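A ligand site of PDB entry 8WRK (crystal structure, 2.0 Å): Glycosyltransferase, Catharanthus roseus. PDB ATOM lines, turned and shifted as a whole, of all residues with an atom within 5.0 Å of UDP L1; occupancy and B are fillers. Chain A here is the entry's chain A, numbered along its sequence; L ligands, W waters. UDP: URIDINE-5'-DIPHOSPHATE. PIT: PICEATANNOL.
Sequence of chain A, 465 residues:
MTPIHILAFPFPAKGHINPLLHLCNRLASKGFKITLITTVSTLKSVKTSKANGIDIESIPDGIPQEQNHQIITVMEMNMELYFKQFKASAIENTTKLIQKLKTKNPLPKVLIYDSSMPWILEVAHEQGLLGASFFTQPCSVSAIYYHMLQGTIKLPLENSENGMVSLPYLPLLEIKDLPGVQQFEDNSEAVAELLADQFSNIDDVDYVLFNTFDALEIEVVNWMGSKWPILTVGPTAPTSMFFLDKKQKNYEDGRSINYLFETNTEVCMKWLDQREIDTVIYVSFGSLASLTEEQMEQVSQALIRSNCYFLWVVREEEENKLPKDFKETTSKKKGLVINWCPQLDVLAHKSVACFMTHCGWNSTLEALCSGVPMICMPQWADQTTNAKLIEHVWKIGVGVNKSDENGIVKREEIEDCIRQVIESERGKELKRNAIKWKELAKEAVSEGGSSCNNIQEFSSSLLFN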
ATOM      1  N   LYS A  14      16.440 -11.099  25.691  1.00  0.00           N
ATOM      2  CA  LYS A  14      17.649 -11.722  26.225  1.00  0.00           C
ATOM      3  C   LYS A  14      18.513 -10.709  26.957  1.00  0.00           C
ATOM      4  O   LYS A  14      19.135 -11.043  27.976  1.00  0.00           O
ATOM      5  CB  LYS A  14      18.432 -12.411  25.106  1.00  0.00           C
ATOM      6  CG  LYS A  14      17.624 -13.528  24.415  1.00  0.00           C
ATOM      7  CD  LYS A  14      18.495 -14.595  23.766  1.00  0.00           C
ATOM      8  CE  LYS A  14      17.629 -15.675  23.102  1.00  0.00           C
ATOM      9  NZ  LYS A  14      16.257 -15.171  22.786  1.00  0.00           N
ATOM     10  N   GLY A  15      18.567  -9.461  26.477  1.00  0.00           N
ATOM     11  CA  GLY A  15      19.367  -8.431  27.129  1.00  0.00           C
ATOM     12  C   GLY A  15      18.850  -8.002  28.482  1.00  0.00           C
ATOM     13  O   GLY A  15      19.561  -7.327  29.229  1.00  0.00           O
ATOM     14  N   ASN A  18      19.155 -12.095  30.600  1.00  0.00           N
ATOM     15  CA  ASN A  18      20.475 -12.617  30.934  1.00  0.00           C
ATOM     16  C   ASN A  18      21.111 -11.924  32.130  1.00  0.00           C
ATOM     17  O   ASN A  18      21.584 -12.637  33.041  1.00  0.00           O
ATOM     18  CB  ASN A  18      21.397 -12.555  29.704  1.00  0.00           C
ATOM     19  CG  ASN A  18      21.030 -13.597  28.638  1.00  0.00           C
ATOM     20  OD1 ASN A  18      20.181 -14.458  28.862  1.00  0.00           O
ATOM     21  ND2 ASN A  18      21.659 -13.487  27.468  1.00  0.00           N
ATOM     22  N   TYR A 259      23.741 -20.105  30.930  1.00  0.00           N
ATOM     23  CA  TYR A 259      22.895 -19.828  29.785  1.00  0.00           C
ATOM     24  C   TYR A 259      21.630 -20.665  29.816  1.00  0.00           C
ATOM     25  O   TYR A 259      21.672 -21.855  30.169  1.00  0.00           O
ATOM     26  CB  TYR A 259      23.630 -20.067  28.449  1.00  0.00           C
ATOM     27  CG  TYR A 259      25.038 -19.539  28.365  1.00  0.00           C
ATOM     28  CD1 TYR A 259      25.302 -18.216  28.002  1.00  0.00           C
ATOM     29  CD2 TYR A 259      26.121 -20.371  28.613  1.00  0.00           C
ATOM     30  CE1 TYR A 259      26.600 -17.741  27.891  1.00  0.00           C
ATOM     31  CE2 TYR A 259      27.420 -19.908  28.508  1.00  0.00           C
ATOM     32  CZ  TYR A 259      27.660 -18.600  28.151  1.00  0.00           C
ATOM     33  OH  TYR A 259      28.963 -18.141  28.055  1.00  0.00           O
ATOM     34  N   THR A 263      23.532 -22.284  23.042  1.00  0.00           N
ATOM     35  CA  THR A 263      24.715 -21.481  22.792  1.00  0.00           C
ATOM     36  C   THR A 263      25.756 -22.193  21.918  1.00  0.00           C
ATOM     37  O   THR A 263      26.821 -21.609  21.676  1.00  0.00           O
ATOM     38  CB  THR A 263      25.365 -21.066  24.111  1.00  0.00           C
ATOM     39  OG1 THR A 263      25.690 -22.234  24.864  1.00  0.00           O
ATOM     40  CG2 THR A 263      24.417 -20.162  24.944  1.00  0.00           C
ATOM     41  N   TYR A 282      35.568 -11.365  17.034  1.00  0.00           N
ATOM     42  CA  TYR A 282      34.229 -11.795  17.413  1.00  0.00           C
ATOM     43  C   TYR A 282      33.238 -10.750  16.923  1.00  0.00           C
ATOM     44  O   TYR A 282      33.423  -9.549  17.167  1.00  0.00           O
ATOM     45  CB  TYR A 282      34.157 -11.990  18.932  1.00  0.00           C
ATOM     46  CG  TYR A 282      32.780 -12.328  19.456  1.00  0.00           C
ATOM     47  CD1 TYR A 282      31.993 -13.296  18.845  1.00  0.00           C
ATOM     48  CD2 TYR A 282      32.259 -11.678  20.579  1.00  0.00           C
ATOM     49  CE1 TYR A 282      30.723 -13.608  19.317  1.00  0.00           C
ATOM     50  CE2 TYR A 282      30.982 -11.965  21.052  1.00  0.00           C
ATOM     51  CZ  TYR A 282      30.220 -12.927  20.420  1.00  0.00           C
ATOM     52  OH  TYR A 282      28.968 -13.212  20.893  1.00  0.00           O
ATOM     53  N   SER A 284      29.073  -9.791  16.696  1.00  0.00           N
ATOM     54  CA  SER A 284      27.689 -10.064  17.073  1.00  0.00           C
ATOM     55  C   SER A 284      26.901  -8.774  17.185  1.00  0.00           C
ATOM     56  O   SER A 284      27.371  -7.790  17.786  1.00  0.00           O
ATOM     57  CB  SER A 284      27.588 -10.843  18.389  1.00  0.00           C
ATOM     58  OG  SER A 284      26.254 -10.910  18.831  1.00  0.00           O
ATOM     59  N   PHE A 285      25.700  -8.773  16.614  1.00  0.00           N
ATOM     60  CA  PHE A 285      24.786  -7.657  16.742  1.00  0.00           C
ATOM     61  C   PHE A 285      23.662  -7.936  17.741  1.00  0.00           C
ATOM     62  O   PHE A 285      22.649  -7.233  17.738  1.00  0.00           O
ATOM     63  CB  PHE A 285      24.263  -7.281  15.356  1.00  0.00           C
ATOM     64  CG  PHE A 285      25.345  -6.702  14.489  1.00  0.00           C
ATOM     65  CD1 PHE A 285      26.261  -7.526  13.839  1.00  0.00           C
ATOM     66  CD2 PHE A 285      25.514  -5.328  14.397  1.00  0.00           C
ATOM     67  CE1 PHE A 285      27.288  -6.995  13.084  1.00  0.00           C
ATOM     68  CE2 PHE A 285      26.541  -4.796  13.642  1.00  0.00           C
ATOM     69  CZ  PHE A 285      27.430  -5.631  12.990  1.00  0.00           C
ATOM     70  N   GLY A 286      23.855  -8.910  18.615  1.00  0.00           N
ATOM     71  CA  GLY A 286      22.966  -9.124  19.738  1.00  0.00           C
ATOM     72  C   GLY A 286      21.752  -9.960  19.373  1.00  0.00           C
ATOM     73  O   GLY A 286      21.733 -10.699  18.387  1.00  0.00           O
ATOM     74  N   SER A 287      20.700  -9.828  20.201  1.00  0.00           N
ATOM     75  CA  SER A 287      19.550 -10.716  20.124  1.00  0.00           C
ATOM     76  C   SER A 287      18.394 -10.143  19.326  1.00  0.00           C
ATOM     77  O   SER A 287      17.507 -10.905  18.930  1.00  0.00           O
ATOM     78  CB  SER A 287      19.054 -11.074  21.535  1.00  0.00           C
ATOM     79  OG  SER A 287      18.360  -9.978  22.113  1.00  0.00           O
ATOM     80  N   LEU A 288      18.393  -8.850  19.086  1.00  0.00           N
ATOM     81  CA  LEU A 288      17.267  -8.156  18.481  1.00  0.00           C
ATOM     82  C   LEU A 288      17.602  -7.519  17.144  1.00  0.00           C
ATOM     83  O   LEU A 288      16.822  -7.642  16.203  1.00  0.00           O
ATOM     84  CB  LEU A 288      16.766  -7.066  19.432  1.00  0.00           C
ATOM     85  CG  LEU A 288      15.778  -7.494  20.510  1.00  0.00           C
ATOM     86  CD1 LEU A 288      15.428  -6.303  21.394  1.00  0.00           C
ATOM     87  CD2 LEU A 288      14.524  -8.110  19.873  1.00  0.00           C
ATOM     88  N   VAL A 313      28.241 -14.289  14.957  1.00  0.00           N
ATOM     89  CA  VAL A 313      26.892 -14.721  15.317  1.00  0.00           C
ATOM     90  C   VAL A 313      25.899 -14.094  14.347  1.00  0.00           C
ATOM     91  O   VAL A 313      25.714 -12.878  14.314  1.00  0.00           O
ATOM     92  CB  VAL A 313      26.548 -14.362  16.761  1.00  0.00           C
ATOM     93  CG1 VAL A 313      25.103 -14.748  17.054  1.00  0.00           C
ATOM     94  CG2 VAL A 313      27.482 -15.063  17.719  1.00  0.00           C
ATOM     95  N   TRP A 340      24.239 -18.693  17.431  1.00  0.00           N
ATOM     96  CA  TRP A 340      24.302 -18.212  18.801  1.00  0.00           C
ATOM     97  C   TRP A 340      25.528 -18.852  19.438  1.00  0.00           C
ATOM     98  O   TRP A 340      25.890 -19.977  19.096  1.00  0.00           O
ATOM     99  CB  TRP A 340      23.014 -18.570  19.579  1.00  0.00           C
ATOM    100  CG  TRP A 340      22.682 -17.648  20.739  1.00  0.00           C
ATOM    101  CD1 TRP A 340      22.610 -17.986  22.065  1.00  0.00           C
ATOM    102  CD2 TRP A 340      22.380 -16.242  20.668  1.00  0.00           C
ATOM    103  NE1 TRP A 340      22.279 -16.874  22.829  1.00  0.00           N
ATOM    104  CE2 TRP A 340      22.133 -15.795  21.995  1.00  0.00           C
ATOM    105  CE3 TRP A 340      22.306 -15.326  19.612  1.00  0.00           C
ATOM    106  CZ2 TRP A 340      21.805 -14.467  22.292  1.00  0.00           C
ATOM    107  CZ3 TRP A 340      22.003 -13.996  19.909  1.00  0.00           C
ATOM    108  CH2 TRP A 340      21.742 -13.578  21.244  1.00  0.00           C
ATOM    109  N   CYS A 341      26.184 -18.132  20.320  1.00  0.00           N
ATOM    110  CA  CYS A 341      27.419 -18.600  20.900  1.00  0.00           C
ATOM    111  C   CYS A 341      27.389 -18.397  22.409  1.00  0.00           C
ATOM    112  O   CYS A 341      26.508 -17.686  22.918  1.00  0.00           O
ATOM    113  CB  CYS A 341      28.630 -17.879  20.270  1.00  0.00           C
ATOM    114  SG  CYS A 341      29.028 -16.281  21.005  1.00  0.00           S
ATOM    115  N   PRO A 342      28.302 -19.036  23.155  1.00  0.00           N
ATOM    116  CA  PRO A 342      28.392 -18.751  24.592  1.00  0.00           C
ATOM    117  C   PRO A 342      29.179 -17.472  24.796  1.00  0.00           C
ATOM    118  O   PRO A 342      30.395 -17.532  24.954  1.00  0.00           O
ATOM    119  CB  PRO A 342      29.088 -19.989  25.159  1.00  0.00           C
ATOM    120  CG  PRO A 342      30.005 -20.451  24.016  1.00  0.00           C
ATOM    121  CD  PRO A 342      29.295 -20.051  22.726  1.00  0.00           C
ATOM    122  N   GLN A 343      28.509 -16.316  24.733  1.00  0.00           N
ATOM    123  CA  GLN A 343      29.244 -15.062  24.579  1.00  0.00           C
ATOM    124  C   GLN A 343      30.260 -14.853  25.698  1.00  0.00           C
ATOM    125  O   GLN A 343      31.363 -14.365  25.438  1.00  0.00           O
ATOM    126  CB  GLN A 343      28.296 -13.859  24.500  1.00  0.00           C
ATOM    127  CG  GLN A 343      29.051 -12.503  24.549  1.00  0.00           C
ATOM    128  CD  GLN A 343      28.291 -11.349  23.923  1.00  0.00           C
ATOM    129  OE1 GLN A 343      28.152 -10.281  24.524  1.00  0.00           O
ATOM    130  NE2 GLN A 343      27.796 -11.560  22.713  1.00  0.00           N
ATOM    131  N   LEU A 344      29.911 -15.216  26.935  1.00  0.00           N
ATOM    132  CA  LEU A 344      30.847 -15.019  28.040  1.00  0.00           C
ATOM    133  C   LEU A 344      32.124 -15.822  27.824  1.00  0.00           C
ATOM    134  O   LEU A 344      33.233 -15.320  28.056  1.00  0.00           O
ATOM    135  CB  LEU A 344      30.205 -15.418  29.375  1.00  0.00           C
ATOM    136  CG  LEU A 344      28.902 -14.685  29.763  1.00  0.00           C
ATOM    137  CD1 LEU A 344      28.338 -15.216  31.083  1.00  0.00           C
ATOM    138  CD2 LEU A 344      29.136 -13.180  29.818  1.00  0.00           C
ATOM    139  N   HIS A 358      27.174  -4.364  18.267  1.00  0.00           N
ATOM    140  CA  HIS A 358      26.151  -3.310  18.201  1.00  0.00           C
ATOM    141  C   HIS A 358      26.117  -2.425  19.453  1.00  0.00           C
ATOM    142  O   HIS A 358      25.328  -1.477  19.497  1.00  0.00           O
ATOM    143  CB  HIS A 358      24.757  -3.927  17.967  1.00  0.00           C
ATOM    144  CG  HIS A 358      24.154  -4.574  19.181  1.00  0.00           C
ATOM    145  ND1 HIS A 358      24.843  -5.460  19.986  1.00  0.00           N
ATOM    146  CD2 HIS A 358      22.902  -4.493  19.709  1.00  0.00           C
ATOM    147  CE1 HIS A 358      24.059  -5.874  20.963  1.00  0.00           C
ATOM    148  NE2 HIS A 358      22.875  -5.308  20.814  1.00  0.00           N
ATOM    149  N   GLY A 360      25.085  -3.054  22.547  1.00  0.00           N
ATOM    150  CA  GLY A 360      24.146  -3.298  23.635  1.00  0.00           C
ATOM    151  C   GLY A 360      24.894  -3.275  24.961  1.00  0.00           C
ATOM    152  O   GLY A 360      26.088  -3.522  25.013  1.00  0.00           O
ATOM    153  N   TRP A 361      24.178  -2.935  26.035  1.00  0.00           N
ATOM    154  CA  TRP A 361      24.886  -2.746  27.301  1.00  0.00           C
ATOM    155  C   TRP A 361      25.544  -4.031  27.798  1.00  0.00           C
ATOM    156  O   TRP A 361      26.653  -3.993  28.334  1.00  0.00           O
ATOM    157  CB  TRP A 361      23.956  -2.191  28.380  1.00  0.00           C
ATOM    158  CG  TRP A 361      24.742  -2.023  29.671  1.00  0.00           C
ATOM    159  CD1 TRP A 361      24.441  -2.559  30.879  1.00  0.00           C
ATOM    160  CD2 TRP A 361      25.983  -1.306  29.840  1.00  0.00           C
ATOM    161  NE1 TRP A 361      25.396  -2.201  31.803  1.00  0.00           N
ATOM    162  CE2 TRP A 361      26.357  -1.438  31.188  1.00  0.00           C
ATOM    163  CE3 TRP A 361      26.813  -0.564  28.975  1.00  0.00           C
ATOM    164  CZ2 TRP A 361      27.528  -0.857  31.710  1.00  0.00           C
ATOM    165  CZ3 TRP A 361      27.976   0.019  29.502  1.00  0.00           C
ATOM    166  CH2 TRP A 361      28.319  -0.145  30.852  1.00  0.00           C
ATOM    167  N   ASN A 362      24.858  -5.167  27.717  1.00  0.00           N
ATOM    168  CA  ASN A 362      25.464  -6.407  28.185  1.00  0.00           C
ATOM    169  C   ASN A 362      26.727  -6.725  27.377  1.00  0.00           C
ATOM    170  O   ASN A 362      27.770  -7.091  27.945  1.00  0.00           O
ATOM    171  CB  ASN A 362      24.461  -7.569  28.090  1.00  0.00           C
ATOM    172  CG  ASN A 362      23.252  -7.380  29.011  1.00  0.00           C
ATOM    173  OD1 ASN A 362      23.329  -7.574  30.229  1.00  0.00           O
ATOM    174  ND2 ASN A 362      22.111  -6.997  28.426  1.00  0.00           N
ATOM    175  N   SER A 363      26.657  -6.608  26.057  1.00  0.00           N
ATOM    176  CA  SER A 363      27.849  -6.903  25.256  1.00  0.00           C
ATOM    177  C   SER A 363      28.965  -5.936  25.576  1.00  0.00           C
ATOM    178  O   SER A 363      30.137  -6.340  25.697  1.00  0.00           O
ATOM    179  CB  SER A 363      27.482  -6.875  23.774  1.00  0.00           C
ATOM    180  OG  SER A 363      26.779  -8.070  23.434  1.00  0.00           O
ATOM    181  N   THR A 364      28.621  -4.658  25.779  1.00  0.00           N
ATOM    182  CA  THR A 364      29.607  -3.648  26.163  1.00  0.00           C
ATOM    183  C   THR A 364      30.284  -4.010  27.483  1.00  0.00           C
ATOM    184  O   THR A 364      31.519  -4.074  27.573  1.00  0.00           O
ATOM    185  CB  THR A 364      28.910  -2.275  26.298  1.00  0.00           C
ATOM    186  OG1 THR A 364      28.377  -1.898  25.022  1.00  0.00           O
ATOM    187  CG2 THR A 364      29.901  -1.196  26.810  1.00  0.00           C
ATOM    188  N   GLU A 366      30.252  -6.883  29.186  1.00  0.00           N
ATOM    189  CA  GLU A 366      30.921  -8.174  29.176  1.00  0.00           C
ATOM    190  C   GLU A 366      32.288  -8.078  28.485  1.00  0.00           C
ATOM    191  O   GLU A 366      33.266  -8.688  28.934  1.00  0.00           O
ATOM    192  CB  GLU A 366      30.029  -9.232  28.498  1.00  0.00           C
ATOM    193  CG  GLU A 366      28.787  -9.603  29.366  1.00  0.00           C
ATOM    194  CD  GLU A 366      27.654 -10.263  28.587  1.00  0.00           C
ATOM    195  OE1 GLU A 366      27.851 -10.626  27.407  1.00  0.00           O
ATOM    196  OE2 GLU A 366      26.559 -10.425  29.186  1.00  0.00           O
ATOM    197  N   GLN A 383      22.361   2.077  22.366  1.00  0.00           N
ATOM    198  CA  GLN A 383      23.615   1.593  21.802  1.00  0.00           C
ATOM    199  C   GLN A 383      24.462   2.744  21.280  1.00  0.00           C
ATOM    200  O   GLN A 383      25.704   2.698  21.374  1.00  0.00           O
ATOM    201  CB  GLN A 383      23.308   0.595  20.678  1.00  0.00           C
ATOM    202  CG  GLN A 383      22.539  -0.654  21.129  1.00  0.00           C
ATOM    203  CD  GLN A 383      21.669  -1.251  20.019  1.00  0.00           C
ATOM    204  OE1 GLN A 383      21.973  -1.111  18.837  1.00  0.00           O
ATOM    205  NE2 GLN A 383      20.593  -1.939  20.413  1.00  0.00           N
HETATM  206  N1  UDP L   1      24.649 -13.345  23.671  1.00  0.00           N
HETATM  207  C2  UDP L   1      24.972 -14.628  23.684  1.00  0.00           C
HETATM  208  N3  UDP L   1      25.372 -15.280  22.617  1.00  0.00           N
HETATM  209  C4  UDP L   1      25.411 -14.642  21.463  1.00  0.00           C
HETATM  210  C5  UDP L   1      25.084 -13.310  21.377  1.00  0.00           C
HETATM  211  C6  UDP L   1      24.679 -12.655  22.541  1.00  0.00           C
HETATM  212  O2  UDP L   1      24.951 -15.323  24.877  1.00  0.00           O
HETATM  213  O4  UDP L   1      25.815 -15.349  20.339  1.00  0.00           O
HETATM  214  C1' UDP L   1      24.172 -12.687  24.892  1.00  0.00           C
HETATM  215  C2' UDP L   1      25.105 -11.618  25.450  1.00  0.00           C
HETATM  216  O2' UDP L   1      25.988 -12.210  26.333  1.00  0.00           O
HETATM  217  C3' UDP L   1      24.075 -10.701  26.151  1.00  0.00           C
HETATM  218  C4' UDP L   1      22.986 -10.710  25.385  1.00  0.00           C
HETATM  219  O4' UDP L   1      23.030 -12.089  24.573  1.00  0.00           O
HETATM  220  O3' UDP L   1      23.720 -11.284  27.471  1.00  0.00           O
HETATM  221  C5' UDP L   1      22.948  -9.561  24.399  1.00  0.00           C
HETATM  222  O5' UDP L   1      22.584  -8.449  25.167  1.00  0.00           O
HETATM  223  PA  UDP L   1      22.956  -6.922  24.678  1.00  0.00           P
HETATM  224  O1A UDP L   1      22.537  -5.971  25.796  1.00  0.00           O
HETATM  225  O2A UDP L   1      24.441  -6.833  24.395  1.00  0.00           O
HETATM  226  O3A UDP L   1      22.150  -6.559  23.314  1.00  0.00           O
HETATM  227  PB  UDP L   1      20.599  -6.841  22.927  1.00  0.00           P
HETATM  228  O1B UDP L   1      19.693  -6.587  24.116  1.00  0.00           O
HETATM  229  O2B UDP L   1      20.488  -8.285  22.477  1.00  0.00           O
HETATM  230  O3B UDP L   1      20.268  -5.868  21.825  1.00  0.00           O
HETATM  231  C1  PIT L   2      12.845  -2.170  25.347  1.00  0.00           C
HETATM  232  C2  PIT L   2      13.100  -1.242  24.352  1.00  0.00           C
HETATM  233  C3  PIT L   2      14.159  -1.443  23.484  1.00  0.00           C
HETATM  234  C4  PIT L   2      14.961  -2.570  23.602  1.00  0.00           C
HETATM  235  C5  PIT L   2      14.692  -3.523  24.581  1.00  0.00           C
HETATM  236  C6  PIT L   2      13.635  -3.304  25.467  1.00  0.00           C
HETATM  237  C7  PIT L   2      15.556  -4.714  24.692  1.00  0.00           C
HETATM  238  C8  PIT L   2      16.799  -4.814  24.219  1.00  0.00           C
HETATM  239  C9  PIT L   2      17.994  -4.214  24.819  1.00  0.00           C
HETATM  240  C10 PIT L   2      18.045  -4.024  26.204  1.00  0.00           C
HETATM  241  C11 PIT L   2      19.153  -3.472  26.814  1.00  0.00           C
HETATM  242  C12 PIT L   2      20.243  -3.097  26.030  1.00  0.00           C
HETATM  243  C13 PIT L   2      20.213  -3.286  24.659  1.00  0.00           C
HETATM  244  C14 PIT L   2      19.091  -3.838  24.067  1.00  0.00           C
HETATM  245  O1  PIT L   2      21.331  -2.532  26.620  1.00  0.00           O
HETATM  246  O2  PIT L   2      14.415  -0.528  22.497  1.00  0.00           O
HETATM  247  O3  PIT L   2      11.794  -1.970  26.210  1.00  0.00           O
HETATM  248  OAD PIT L   2      19.171  -3.277  28.181  1.00  0.00           O
HETATM  249  O   HOH W   1      26.178  -9.934  21.322  1.00  0.00           O
HETATM  250  O   HOH W   2      20.399  -6.695  19.306  1.00  0.00           O
HETATM  251  O   HOH W   3      25.770 -14.793  27.533  1.00  0.00           O
HETATM  252  O   HOH W   4      17.322  -7.689  24.537  1.00  0.00           O
HETATM  253  O   HOH W   5      25.290 -12.674  29.519  1.00  0.00           O
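The side-chain carboxylate (OE1) of Glu 366 is in hydrogen-bond range of an oxygen (O2') of UDP L1. The backbone NH (N) of Cys 341 is in hydrogen-bond range of an oxygen (O4) of UDP L1 (2.8 Å). The backbone carbonyl oxygen (O) of Cys 341 sits at hydrogen-bond distance from a nitrogen (N3) of UDP L1 (2.7 Å). The side-chain sulfur (SG) of Cys 341 lies within hydrogen-bond range of an oxygen (O4) of UDP L1, 3.4 Å away. O2B of UDP L1 sits at hydrogen-bond distance from N of Ser 287, at 2.8 Å. O2B of UDP L1 lies within hydrogen-bond range of OG of Ser 287, at 2.7 Å. The backbone NH (N) of Ser 363 sits at hydrogen-bond distance from an oxygen (O2A) of UDP L1, at 2.8 Å. O2A of UDP L1 lies within hydrogen-bond range of OG of Ser 363. A ring nitrogen (NE2) of His 358 sits at hydrogen-bond distance from an oxygen (O3B) of UDP L1. The backbone NH of Asn 362 sits at hydrogen-bond distance from an oxygen (O1A) of UDP L1 (3.1 Å). An oxygen (O1A) of UDP L1 is in hydrogen-bond range of the side-chain amide nitrogen (ND2) of Asn 362. An oxygen (O3') of UDP L1 sits at hydrogen-bond distance from the side-chain amide nitrogen of Asn 18. The side-chain amide oxygen (OE1) of Gln 343 sits close to an oxygen (O2') of UDP L1, at 3.4 Å. The backbone NH (N) of Trp 361 sits at hydrogen-bond distance from an oxygen (O1A) of UDP L1. An oxygen (O1) of PIT L2 lies within hydrogen-bond range of the backbone NH (N) of Trp 361, at 2.9 Å.
The side-chain sulfur (SG) of Cys 341 sits close to the backbone NH (N) of Gln 343, 3.8 Å away. The side-chain sulfur (SG) of Cys 341 lies within hydrogen-bond range of the side-chain hydroxyl (OH) of Tyr 282, at 3.1 Å. The backbone carbonyl oxygen of Ser 284 is in hydrogen-bond range of the backbone NH of His 358 (3.5 Å). OE1 of Gln 383 sits close to O of His 358. The backbone carbonyl oxygen (O) of Gly 15 sits at hydrogen-bond distance from the side-chain amide nitrogen (ND2) of Asn 362, at 2.7 Å. OH of Tyr 282 lies within hydrogen-bond range of NE2 of Gln 343 (2.7 Å). The side-chain hydroxyl of Thr 364 is in hydrogen-bond range of the backbone carbonyl oxygen of Gly 360 (2.8 Å). The backbone NH of Gly 286 sits at hydrogen-bond distance from the side-chain hydroxyl of Ser 284, 3.1 Å away.
NE1 of Trp 340 sits close to N3 of UDP L1, 3.5 Å away. Residues that only touch UDP L1: Val 313, Gly 15, Gly 360, Ser 284, Gly 286 and Tyr 282. 16 residues have an atom within 4 Å of UDP L1: Gly 15, Asn 18, Tyr 282, Ser 284, Gly 286, Ser 287, Val 313, Trp 340, Cys 341, Gln 343, His 358, Gly 360, Trp 361, Asn 362, Ser 363 and Glu 366.
Water W4 lies within hydrogen-bond range of an oxygen (O1B) of UDP L1, the backbone NH (N) of Gly 15 and the side-chain hydroxyl (OG) of Ser 287. Water W2 lies within hydrogen-bond range of O3B of UDP L1 (2.7 Å), O of Phe 285 (2.8 Å), N of Leu 288 (3.0 Å), NE2 of His 358 (3.2 Å) and N of Ser 287 (3.3 Å). Water W5 lies within hydrogen-bond range of OE2 of Glu 366 and O3' of UDP L1. Water W1 lies within hydrogen-bond range of OG of Ser 284, NE2 of Gln 343 and OG of Ser 363.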
